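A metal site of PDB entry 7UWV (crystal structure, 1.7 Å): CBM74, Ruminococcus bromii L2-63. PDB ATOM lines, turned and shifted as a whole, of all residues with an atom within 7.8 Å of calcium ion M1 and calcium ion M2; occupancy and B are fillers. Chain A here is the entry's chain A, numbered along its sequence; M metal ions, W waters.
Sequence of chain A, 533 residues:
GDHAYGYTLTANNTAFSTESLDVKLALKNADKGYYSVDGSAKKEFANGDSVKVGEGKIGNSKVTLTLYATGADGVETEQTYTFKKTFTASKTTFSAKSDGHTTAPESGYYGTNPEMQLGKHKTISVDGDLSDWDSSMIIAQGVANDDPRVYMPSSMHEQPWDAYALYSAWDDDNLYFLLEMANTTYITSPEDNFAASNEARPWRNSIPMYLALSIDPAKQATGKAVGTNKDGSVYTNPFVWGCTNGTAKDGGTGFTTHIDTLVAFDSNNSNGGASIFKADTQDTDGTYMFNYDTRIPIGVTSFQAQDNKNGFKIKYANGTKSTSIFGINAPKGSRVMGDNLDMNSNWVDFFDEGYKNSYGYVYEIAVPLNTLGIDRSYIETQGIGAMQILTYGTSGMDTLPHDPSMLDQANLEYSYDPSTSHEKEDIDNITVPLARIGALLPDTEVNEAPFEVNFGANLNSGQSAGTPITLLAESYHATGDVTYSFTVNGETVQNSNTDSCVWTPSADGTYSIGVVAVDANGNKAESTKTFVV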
ATOM      1  N   PRO A 148      -9.070 -18.581 -13.441  1.00  0.00           N
ATOM      2  CA  PRO A 148      -7.681 -18.567 -12.977  1.00  0.00           C
ATOM      3  C   PRO A 148      -6.904 -19.902 -13.012  1.00  0.00           C
ATOM      4  O   PRO A 148      -5.696 -19.864 -13.216  1.00  0.00           O
ATOM      5  CB  PRO A 148      -7.816 -18.075 -11.530  1.00  0.00           C
ATOM      6  CG  PRO A 148      -9.023 -17.156 -11.603  1.00  0.00           C
ATOM      7  CD  PRO A 148      -9.980 -17.941 -12.476  1.00  0.00           C
ATOM      8  N   ASP A 250      -8.571 -14.830   3.648  1.00  0.00           N
ATOM      9  CA  ASP A 250      -8.518 -15.396   2.271  1.00  0.00           C
ATOM     10  C   ASP A 250      -9.151 -14.393   1.290  1.00  0.00           C
ATOM     11  O   ASP A 250      -9.735 -14.821   0.288  1.00  0.00           O
ATOM     12  CB  ASP A 250      -9.180 -16.769   2.239  1.00  0.00           C
ATOM     13  CG  ASP A 250      -8.494 -17.784   3.146  1.00  0.00           C
ATOM     14  OD1 ASP A 250      -7.272 -17.642   3.382  1.00  0.00           O
ATOM     15  OD2 ASP A 250      -9.194 -18.703   3.597  1.00  0.00           O
ATOM     16  N   GLY A 251      -9.001 -13.094   1.583  1.00  0.00           N
ATOM     17  CA  GLY A 251      -9.291 -12.016   0.619  1.00  0.00           C
ATOM     18  C   GLY A 251     -10.775 -11.863   0.318  1.00  0.00           C
ATOM     19  O   GLY A 251     -11.614 -12.260   1.146  1.00  0.00           O
ATOM     20  N   GLY A 252     -11.081 -11.301  -0.849  1.00  0.00           N
ATOM     21  CA  GLY A 252     -12.413 -10.817  -1.204  1.00  0.00           C
ATOM     22  C   GLY A 252     -12.345  -9.907  -2.413  1.00  0.00           C
ATOM     23  O   GLY A 252     -11.239  -9.780  -2.994  1.00  0.00           O
ATOM     24  N   THR A 253     -13.469  -9.298  -2.774  1.00  0.00           N
ATOM     25  CA  THR A 253     -13.597  -8.390  -3.942  1.00  0.00           C
ATOM     26  C   THR A 253     -14.010  -7.005  -3.435  1.00  0.00           C
ATOM     27  O   THR A 253     -15.062  -6.915  -2.780  1.00  0.00           O
ATOM     28  CB  THR A 253     -14.571  -8.937  -4.985  1.00  0.00           C
ATOM     29  OG1 THR A 253     -14.148 -10.261  -5.309  1.00  0.00           O
ATOM     30  CG2 THR A 253     -14.637  -8.075  -6.220  1.00  0.00           C
ATOM     31  N   LEU A 390     -18.229 -14.389  -9.755  1.00  0.00           N
ATOM     32  CA  LEU A 390     -18.027 -15.774  -9.270  1.00  0.00           C
ATOM     33  C   LEU A 390     -16.845 -15.800  -8.317  1.00  0.00           C
ATOM     34  O   LEU A 390     -15.886 -15.033  -8.514  1.00  0.00           O
ATOM     35  CB  LEU A 390     -17.751 -16.708 -10.453  1.00  0.00           C
ATOM     36  CG  LEU A 390     -18.875 -16.837 -11.482  1.00  0.00           C
ATOM     37  CD1 LEU A 390     -18.476 -17.852 -12.528  1.00  0.00           C
ATOM     38  CD2 LEU A 390     -20.188 -17.237 -10.818  1.00  0.00           C
ATOM     39  N   THR A 391     -16.903 -16.690  -7.336  1.00  0.00           N
ATOM     40  CA  THR A 391     -15.828 -16.972  -6.367  1.00  0.00           C
ATOM     41  C   THR A 391     -15.601 -18.481  -6.308  1.00  0.00           C
ATOM     42  O   THR A 391     -16.371 -19.244  -6.938  1.00  0.00           O
ATOM     43  CB  THR A 391     -16.177 -16.446  -4.971  1.00  0.00           C
ATOM     44  OG1 THR A 391     -17.080 -17.359  -4.350  1.00  0.00           O
ATOM     45  CG2 THR A 391     -16.779 -15.050  -4.987  1.00  0.00           C
ATOM     46  N   THR A 394     -14.368 -17.087  -1.352  1.00  0.00           N
ATOM     47  CA  THR A 394     -14.073 -15.729  -0.819  1.00  0.00           C
ATOM     48  C   THR A 394     -13.793 -14.782  -1.983  1.00  0.00           C
ATOM     49  O   THR A 394     -14.734 -14.083  -2.415  1.00  0.00           O
ATOM     50  CB  THR A 394     -12.932 -15.782   0.205  1.00  0.00           C
ATOM     51  OG1 THR A 394     -11.795 -16.406  -0.389  1.00  0.00           O
ATOM     52  CG2 THR A 394     -13.324 -16.503   1.480  1.00  0.00           C
ATOM     53  N   SER A 395     -12.558 -14.802  -2.503  1.00  0.00           N
ATOM     54  CA  SER A 395     -12.059 -13.898  -3.572  1.00  0.00           C
ATOM     55  C   SER A 395     -12.747 -14.213  -4.913  1.00  0.00           C
ATOM     56  O   SER A 395     -13.151 -15.374  -5.149  1.00  0.00           O
ATOM     57  CB  SER A 395     -10.561 -13.985  -3.694  1.00  0.00           C
ATOM     58  OG  SER A 395     -10.037 -12.991  -4.579  1.00  0.00           O
ATOM     59  N   GLY A 396     -12.793 -13.213  -5.778  1.00  0.00           N
ATOM     60  CA  GLY A 396     -13.288 -13.329  -7.158  1.00  0.00           C
ATOM     61  C   GLY A 396     -12.435 -14.272  -7.994  1.00  0.00           C
ATOM     62  O   GLY A 396     -11.202 -14.361  -7.753  1.00  0.00           O
ATOM     63  N   MET A 397     -13.072 -14.945  -8.950  1.00  0.00           N
ATOM     64  CA  MET A 397     -12.397 -15.826  -9.930  1.00  0.00           C
ATOM     65  C   MET A 397     -12.721 -15.366 -11.358  1.00  0.00           C
ATOM     66  O   MET A 397     -11.828 -15.495 -12.218  1.00  0.00           O
ATOM     67  CB  MET A 397     -12.857 -17.281  -9.751  1.00  0.00           C
ATOM     68  CG  MET A 397     -12.523 -17.831  -8.372  1.00  0.00           C
ATOM     69  SD  MET A 397     -10.757 -18.184  -8.218  1.00  0.00           S
ATOM     70  CE  MET A 397     -10.669 -19.817  -8.942  1.00  0.00           C
ATOM     71  N   ASP A 398     -13.941 -14.893 -11.617  1.00  0.00           N
ATOM     72  CA  ASP A 398     -14.388 -14.466 -12.967  1.00  0.00           C
ATOM     73  C   ASP A 398     -15.526 -13.461 -12.757  1.00  0.00           C
ATOM     74  O   ASP A 398     -16.243 -13.587 -11.762  1.00  0.00           O
ATOM     75  CB  ASP A 398     -14.793 -15.665 -13.837  1.00  0.00           C
ATOM     76  CG  ASP A 398     -14.838 -15.412 -15.347  1.00  0.00           C
ATOM     77  OD1 ASP A 398     -14.772 -14.239 -15.746  1.00  0.00           O
ATOM     78  OD2 ASP A 398     -14.985 -16.410 -16.118  1.00  0.00           O
ATOM     79  N   ASP A 403     -12.972  -8.307 -15.587  1.00  0.00           N
ATOM     80  CA  ASP A 403     -12.047  -7.340 -14.953  1.00  0.00           C
ATOM     81  C   ASP A 403     -10.677  -8.008 -14.819  1.00  0.00           C
ATOM     82  O   ASP A 403     -10.598  -9.154 -14.384  1.00  0.00           O
ATOM     83  CB  ASP A 403     -12.609  -6.867 -13.620  1.00  0.00           C
ATOM     84  CG  ASP A 403     -11.815  -5.737 -12.985  1.00  0.00           C
ATOM     85  OD1 ASP A 403     -12.332  -4.593 -12.968  1.00  0.00           O
ATOM     86  OD2 ASP A 403     -10.690  -6.016 -12.509  1.00  0.00           O
ATOM     87  N   PRO A 404      -9.577  -7.314 -15.184  1.00  0.00           N
ATOM     88  CA  PRO A 404      -8.245  -7.920 -15.167  1.00  0.00           C
ATOM     89  C   PRO A 404      -7.755  -8.305 -13.762  1.00  0.00           C
ATOM     90  O   PRO A 404      -6.841  -9.106 -13.692  1.00  0.00           O
ATOM     91  CB  PRO A 404      -7.343  -6.837 -15.775  1.00  0.00           C
ATOM     92  CG  PRO A 404      -8.093  -5.538 -15.548  1.00  0.00           C
ATOM     93  CD  PRO A 404      -9.549  -5.913 -15.635  1.00  0.00           C
ATOM     94  N   SER A 405      -8.380  -7.784 -12.708  1.00  0.00           N
ATOM     95  CA  SER A 405      -8.033  -8.148 -11.305  1.00  0.00           C
ATOM     96  C   SER A 405      -8.409  -9.616 -11.036  1.00  0.00           C
ATOM     97  O   SER A 405      -7.942 -10.186 -10.036  1.00  0.00           O
ATOM     98  CB  SER A 405      -8.677  -7.219 -10.300  1.00  0.00           C
ATOM     99  OG  SER A 405     -10.085  -7.390 -10.275  1.00  0.00           O
ATOM    100  N   MET A 406      -9.194 -10.232 -11.920  1.00  0.00           N
ATOM    101  CA  MET A 406      -9.520 -11.673 -11.810  1.00  0.00           C
ATOM    102  C   MET A 406      -8.307 -12.538 -12.186  1.00  0.00           C
ATOM    103  O   MET A 406      -8.316 -13.726 -11.809  1.00  0.00           O
ATOM    104  CB  MET A 406     -10.706 -12.057 -12.697  1.00  0.00           C
ATOM    105  CG  MET A 406     -12.019 -11.444 -12.255  1.00  0.00           C
ATOM    106  SD  MET A 406     -12.493 -11.848 -10.543  1.00  0.00           S
ATOM    107  CE  MET A 406     -12.324 -10.226  -9.804  1.00  0.00           C
ATOM    108  N   LEU A 407      -7.310 -11.997 -12.905  1.00  0.00           N
ATOM    109  CA  LEU A 407      -6.191 -12.816 -13.456  1.00  0.00           C
ATOM    110  C   LEU A 407      -4.818 -12.269 -13.078  1.00  0.00           C
ATOM    111  O   LEU A 407      -3.818 -12.879 -13.507  1.00  0.00           O
ATOM    112  CB  LEU A 407      -6.372 -12.895 -14.978  1.00  0.00           C
ATOM    113  CG  LEU A 407      -7.574 -13.726 -15.417  1.00  0.00           C
ATOM    114  CD1 LEU A 407      -7.740 -13.724 -16.940  1.00  0.00           C
ATOM    115  CD2 LEU A 407      -7.474 -15.147 -14.898  1.00  0.00           C
ATOM    116  N   ASP A 408      -4.736 -11.200 -12.265  1.00  0.00           N
ATOM    117  CA  ASP A 408      -3.438 -10.518 -12.021  1.00  0.00           C
ATOM    118  C   ASP A 408      -2.512 -11.413 -11.187  1.00  0.00           C
ATOM    119  O   ASP A 408      -1.303 -11.188 -11.238  1.00  0.00           O
ATOM    120  CB  ASP A 408      -3.618  -9.126 -11.394  1.00  0.00           C
ATOM    121  CG  ASP A 408      -4.303  -9.114 -10.036  1.00  0.00           C
ATOM    122  OD1 ASP A 408      -5.008 -10.074  -9.721  1.00  0.00           O
ATOM    123  OD2 ASP A 408      -4.127  -8.111  -9.311  1.00  0.00           O
ATOM    124  N   GLN A 409      -3.059 -12.397 -10.467  1.00  0.00           N
ATOM    125  CA  GLN A 409      -2.243 -13.331  -9.648  1.00  0.00           C
ATOM    126  C   GLN A 409      -2.629 -14.788  -9.955  1.00  0.00           C
ATOM    127  O   GLN A 409      -2.397 -15.644  -9.099  1.00  0.00           O
ATOM    128  CB  GLN A 409      -2.398 -12.952  -8.173  1.00  0.00           C
ATOM    129  CG  GLN A 409      -1.901 -11.533  -7.887  1.00  0.00           C
ATOM    130  CD  GLN A 409      -1.704 -11.272  -6.413  1.00  0.00           C
ATOM    131  OE1 GLN A 409      -0.599 -11.400  -5.906  1.00  0.00           O
ATOM    132  NE2 GLN A 409      -2.772 -10.911  -5.727  1.00  0.00           N
ATOM    133  N   ALA A 410      -3.137 -15.057 -11.157  1.00  0.00           N
ATOM    134  CA  ALA A 410      -3.694 -16.364 -11.559  1.00  0.00           C
ATOM    135  C   ALA A 410      -2.613 -17.444 -11.493  1.00  0.00           C
ATOM    136  O   ALA A 410      -2.953 -18.568 -11.143  1.00  0.00           O
ATOM    137  CB  ALA A 410      -4.303 -16.279 -12.946  1.00  0.00           C
ATOM    138  N   SER A 421      -4.743 -21.985  -7.734  1.00  0.00           N
ATOM    139  CA  SER A 421      -4.463 -20.548  -7.985  1.00  0.00           C
ATOM    140  C   SER A 421      -4.674 -19.674  -6.745  1.00  0.00           C
ATOM    141  O   SER A 421      -5.737 -19.758  -6.110  1.00  0.00           O
ATOM    142  CB  SER A 421      -5.318 -20.053  -9.127  1.00  0.00           C
ATOM    143  OG  SER A 421      -5.038 -18.691  -9.400  1.00  0.00           O
ATOM    144  N   HIS A 422      -3.716 -18.784  -6.481  1.00  0.00           N
ATOM    145  CA  HIS A 422      -3.792 -17.700  -5.460  1.00  0.00           C
ATOM    146  C   HIS A 422      -5.021 -16.812  -5.691  1.00  0.00           C
ATOM    147  O   HIS A 422      -5.464 -16.162  -4.728  1.00  0.00           O
ATOM    148  CB  HIS A 422      -2.488 -16.881  -5.492  1.00  0.00           C
ATOM    149  CG  HIS A 422      -2.397 -15.821  -4.448  1.00  0.00           C
ATOM    150  ND1 HIS A 422      -2.376 -16.118  -3.102  1.00  0.00           N
ATOM    151  CD2 HIS A 422      -2.263 -14.477  -4.551  1.00  0.00           C
ATOM    152  CE1 HIS A 422      -2.252 -15.006  -2.407  1.00  0.00           C
ATOM    153  NE2 HIS A 422      -2.178 -13.979  -3.270  1.00  0.00           N
ATOM    154  N   GLU A 423      -5.574 -16.751  -6.905  1.00  0.00           N
ATOM    155  CA  GLU A 423      -6.791 -15.937  -7.167  1.00  0.00           C
ATOM    156  C   GLU A 423      -7.936 -16.345  -6.232  1.00  0.00           C
ATOM    157  O   GLU A 423      -8.876 -15.548  -6.069  1.00  0.00           O
ATOM    158  CB  GLU A 423      -7.228 -16.030  -8.634  1.00  0.00           C
ATOM    159  CG  GLU A 423      -6.445 -15.099  -9.532  1.00  0.00           C
ATOM    160  CD  GLU A 423      -6.639 -13.619  -9.228  1.00  0.00           C
ATOM    161  OE1 GLU A 423      -7.627 -13.274  -8.529  1.00  0.00           O
ATOM    162  OE2 GLU A 423      -5.796 -12.818  -9.682  1.00  0.00           O
ATOM    163  N   LYS A 424      -7.855 -17.533  -5.616  1.00  0.00           N
ATOM    164  CA  LYS A 424      -8.925 -18.030  -4.713  1.00  0.00           C
ATOM    165  C   LYS A 424      -8.918 -17.245  -3.399  1.00  0.00           C
ATOM    166  O   LYS A 424      -9.965 -17.264  -2.718  1.00  0.00           O
ATOM    167  CB  LYS A 424      -8.771 -19.537  -4.462  1.00  0.00           C
ATOM    168  CG  LYS A 424      -9.061 -20.422  -5.662  1.00  0.00           C
ATOM    169  CD  LYS A 424      -9.179 -21.892  -5.322  1.00  0.00           C
ATOM    170  CE  LYS A 424      -7.913 -22.475  -4.708  1.00  0.00           C
ATOM    171  NZ  LYS A 424      -8.028 -23.936  -4.499  1.00  0.00           N
ATOM    172  N   GLU A 425      -7.792 -16.622  -3.026  1.00  0.00           N
ATOM    173  CA  GLU A 425      -7.558 -16.088  -1.653  1.00  0.00           C
ATOM    174  C   GLU A 425      -7.024 -14.650  -1.668  1.00  0.00           C
ATOM    175  O   GLU A 425      -6.731 -14.164  -0.564  1.00  0.00           O
ATOM    176  CB  GLU A 425      -6.592 -17.011  -0.902  1.00  0.00           C
ATOM    177  CG  GLU A 425      -5.158 -16.936  -1.408  1.00  0.00           C
ATOM    178  CD  GLU A 425      -4.192 -17.912  -0.763  1.00  0.00           C
ATOM    179  OE1 GLU A 425      -4.468 -18.371   0.371  1.00  0.00           O
ATOM    180  OE2 GLU A 425      -3.131 -18.213  -1.402  1.00  0.00           O
ATOM    181  N   ASP A 426      -6.931 -13.984  -2.821  1.00  0.00           N
ATOM    182  CA  ASP A 426      -6.264 -12.651  -2.933  1.00  0.00           C
ATOM    183  C   ASP A 426      -7.306 -11.542  -2.842  1.00  0.00           C
ATOM    184  O   ASP A 426      -8.517 -11.839  -2.756  1.00  0.00           O
ATOM    185  CB  ASP A 426      -5.404 -12.555  -4.198  1.00  0.00           C
ATOM    186  CG  ASP A 426      -6.193 -12.404  -5.485  1.00  0.00           C
ATOM    187  OD1 ASP A 426      -7.333 -12.920  -5.517  1.00  0.00           O
ATOM    188  OD2 ASP A 426      -5.658 -11.788  -6.463  1.00  0.00           O
ATOM    189  N   ILE A 427      -6.864 -10.287  -2.818  1.00  0.00           N
ATOM    190  CA  ILE A 427      -7.784  -9.115  -2.803  1.00  0.00           C
ATOM    191  C   ILE A 427      -7.923  -8.618  -4.235  1.00  0.00           C
ATOM    192  O   ILE A 427      -6.903  -8.206  -4.818  1.00  0.00           O
ATOM    193  CB  ILE A 427      -7.288  -7.988  -1.876  1.00  0.00           C
ATOM    194  CG1 ILE A 427      -7.180  -8.464  -0.424  1.00  0.00           C
ATOM    195  CG2 ILE A 427      -8.197  -6.775  -1.998  1.00  0.00           C
ATOM    196  CD1 ILE A 427      -6.343  -7.569   0.445  1.00  0.00           C
ATOM    197  N   ASP A 428      -9.131  -8.695  -4.786  1.00  0.00           N
ATOM    198  CA  ASP A 428      -9.473  -8.170  -6.131  1.00  0.00           C
ATOM    199  C   ASP A 428     -10.036  -6.755  -5.966  1.00  0.00           C
ATOM    200  O   ASP A 428     -10.633  -6.468  -4.921  1.00  0.00           O
ATOM    201  CB  ASP A 428     -10.476  -9.094  -6.833  1.00  0.00           C
ATOM    202  CG  ASP A 428      -9.990 -10.522  -6.999  1.00  0.00           C
ATOM    203  OD1 ASP A 428      -8.750 -10.724  -7.098  1.00  0.00           O
ATOM    204  OD2 ASP A 428     -10.861 -11.444  -6.996  1.00  0.00           O
ATOM    205  N   ASN A 429      -9.865  -5.890  -6.964  1.00  0.00           N
ATOM    206  CA  ASN A 429     -10.459  -4.536  -6.951  1.00  0.00           C
ATOM    207  C   ASN A 429     -11.011  -4.229  -8.345  1.00  0.00           C
ATOM    208  O   ASN A 429     -10.206  -4.201  -9.293  1.00  0.00           O
ATOM    209  CB  ASN A 429      -9.471  -3.482  -6.459  1.00  0.00           C
ATOM    210  CG  ASN A 429     -10.141  -2.147  -6.236  1.00  0.00           C
ATOM    211  OD1 ASN A 429     -10.313  -1.381  -7.181  1.00  0.00           O
ATOM    212  ND2 ASN A 429     -10.537  -1.850  -5.005  1.00  0.00           N
HETATM  213 CA    CA M   1      -9.278 -13.289  -6.797  1.00  0.00          CA
HETATM  214 CA    CA M   2      -6.741 -10.884  -8.339  1.00  0.00          CA
HETATM  215  O   HOH W   1      -6.218  -8.702  -7.529  1.00  0.00           O
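The side-chain hydroxyl (OG) of Ser 421 lies close to the backbone NH (N) of Glu 423 (3.2 Å). The backbone carbonyl oxygen of Asn 429 is in hydrogen-bond range of the side-chain hydroxyl of Ser 405, 3.3 Å away. The side-chain carboxylate of Asp 426 lies close to the side-chain amide nitrogen of Gln 409 (3.1 Å). OG1 of Thr 253 lies within hydrogen-bond range of N of Gly 396. OG of Ser 405 lies within hydrogen-bond range of OD2 of Asp 403 (2.7 Å). N of Asp 428 sits at hydrogen-bond distance from O of Gly 252, 3.0 Å away. OE2 of Glu 423 lies close to N of Gln 409 (2.9 Å). The backbone carbonyl oxygen (O) of Asp 426 is in hydrogen-bond range of the backbone NH (N) of Gly 252.
Of the 29 residues printed, 5 come within 4 Å of calcium ion M1.
Five residues have an atom within 4 Å of calcium ion M2: Ser 405, Asp 408, Glu 423, Asp 426 and Asp 428.
Calcium ion M1 is bound by OD1 of Asp 426, at 2.4 Å. Calcium ion M1 is bound by OG of Ser 395 (2.4 Å). Calcium ion M1 is bound by OE1 of Glu 423. Calcium ion M1 is bound by O of Gly 396 (2.4 Å). The backbone carbonyl oxygen (O) of Glu 423 binds calcium ion M1. The side-chain carboxylate (OD2) of Asp 428 binds calcium ion M1 (2.4 Å). The side-chain carboxylate (OD1) of Asp 428 binds calcium ion M1.
Calcium ion M2 is bound by O of Ser 405 (2.2 Å). OD2 of Asp 426 binds calcium ion M2 (2.3 Å). Calcium ion M2 is bound by the side-chain carboxylate (OD1) of Asp 408 (2.4 Å). Calcium ion M2 is bound by the side-chain carboxylate (OD1) of Asp 428, at 2.4 Å. Calcium ion M2 is bound by water W1, at 2.4 Å. Calcium ion M2 is bound by the side-chain carboxylate (OE2) of Glu 423, 2.5 Å away. OE1 of Glu 423 binds calcium ion M2 (2.6 Å). Calcium ion M2 has seven donor atoms within binding distance.
Water W1 bridges the side-chain carboxylate (OD2) of Asp 408 (2.8 Å) and the backbone carbonyl oxygen (O) of Ile 427 (2.8 Å).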
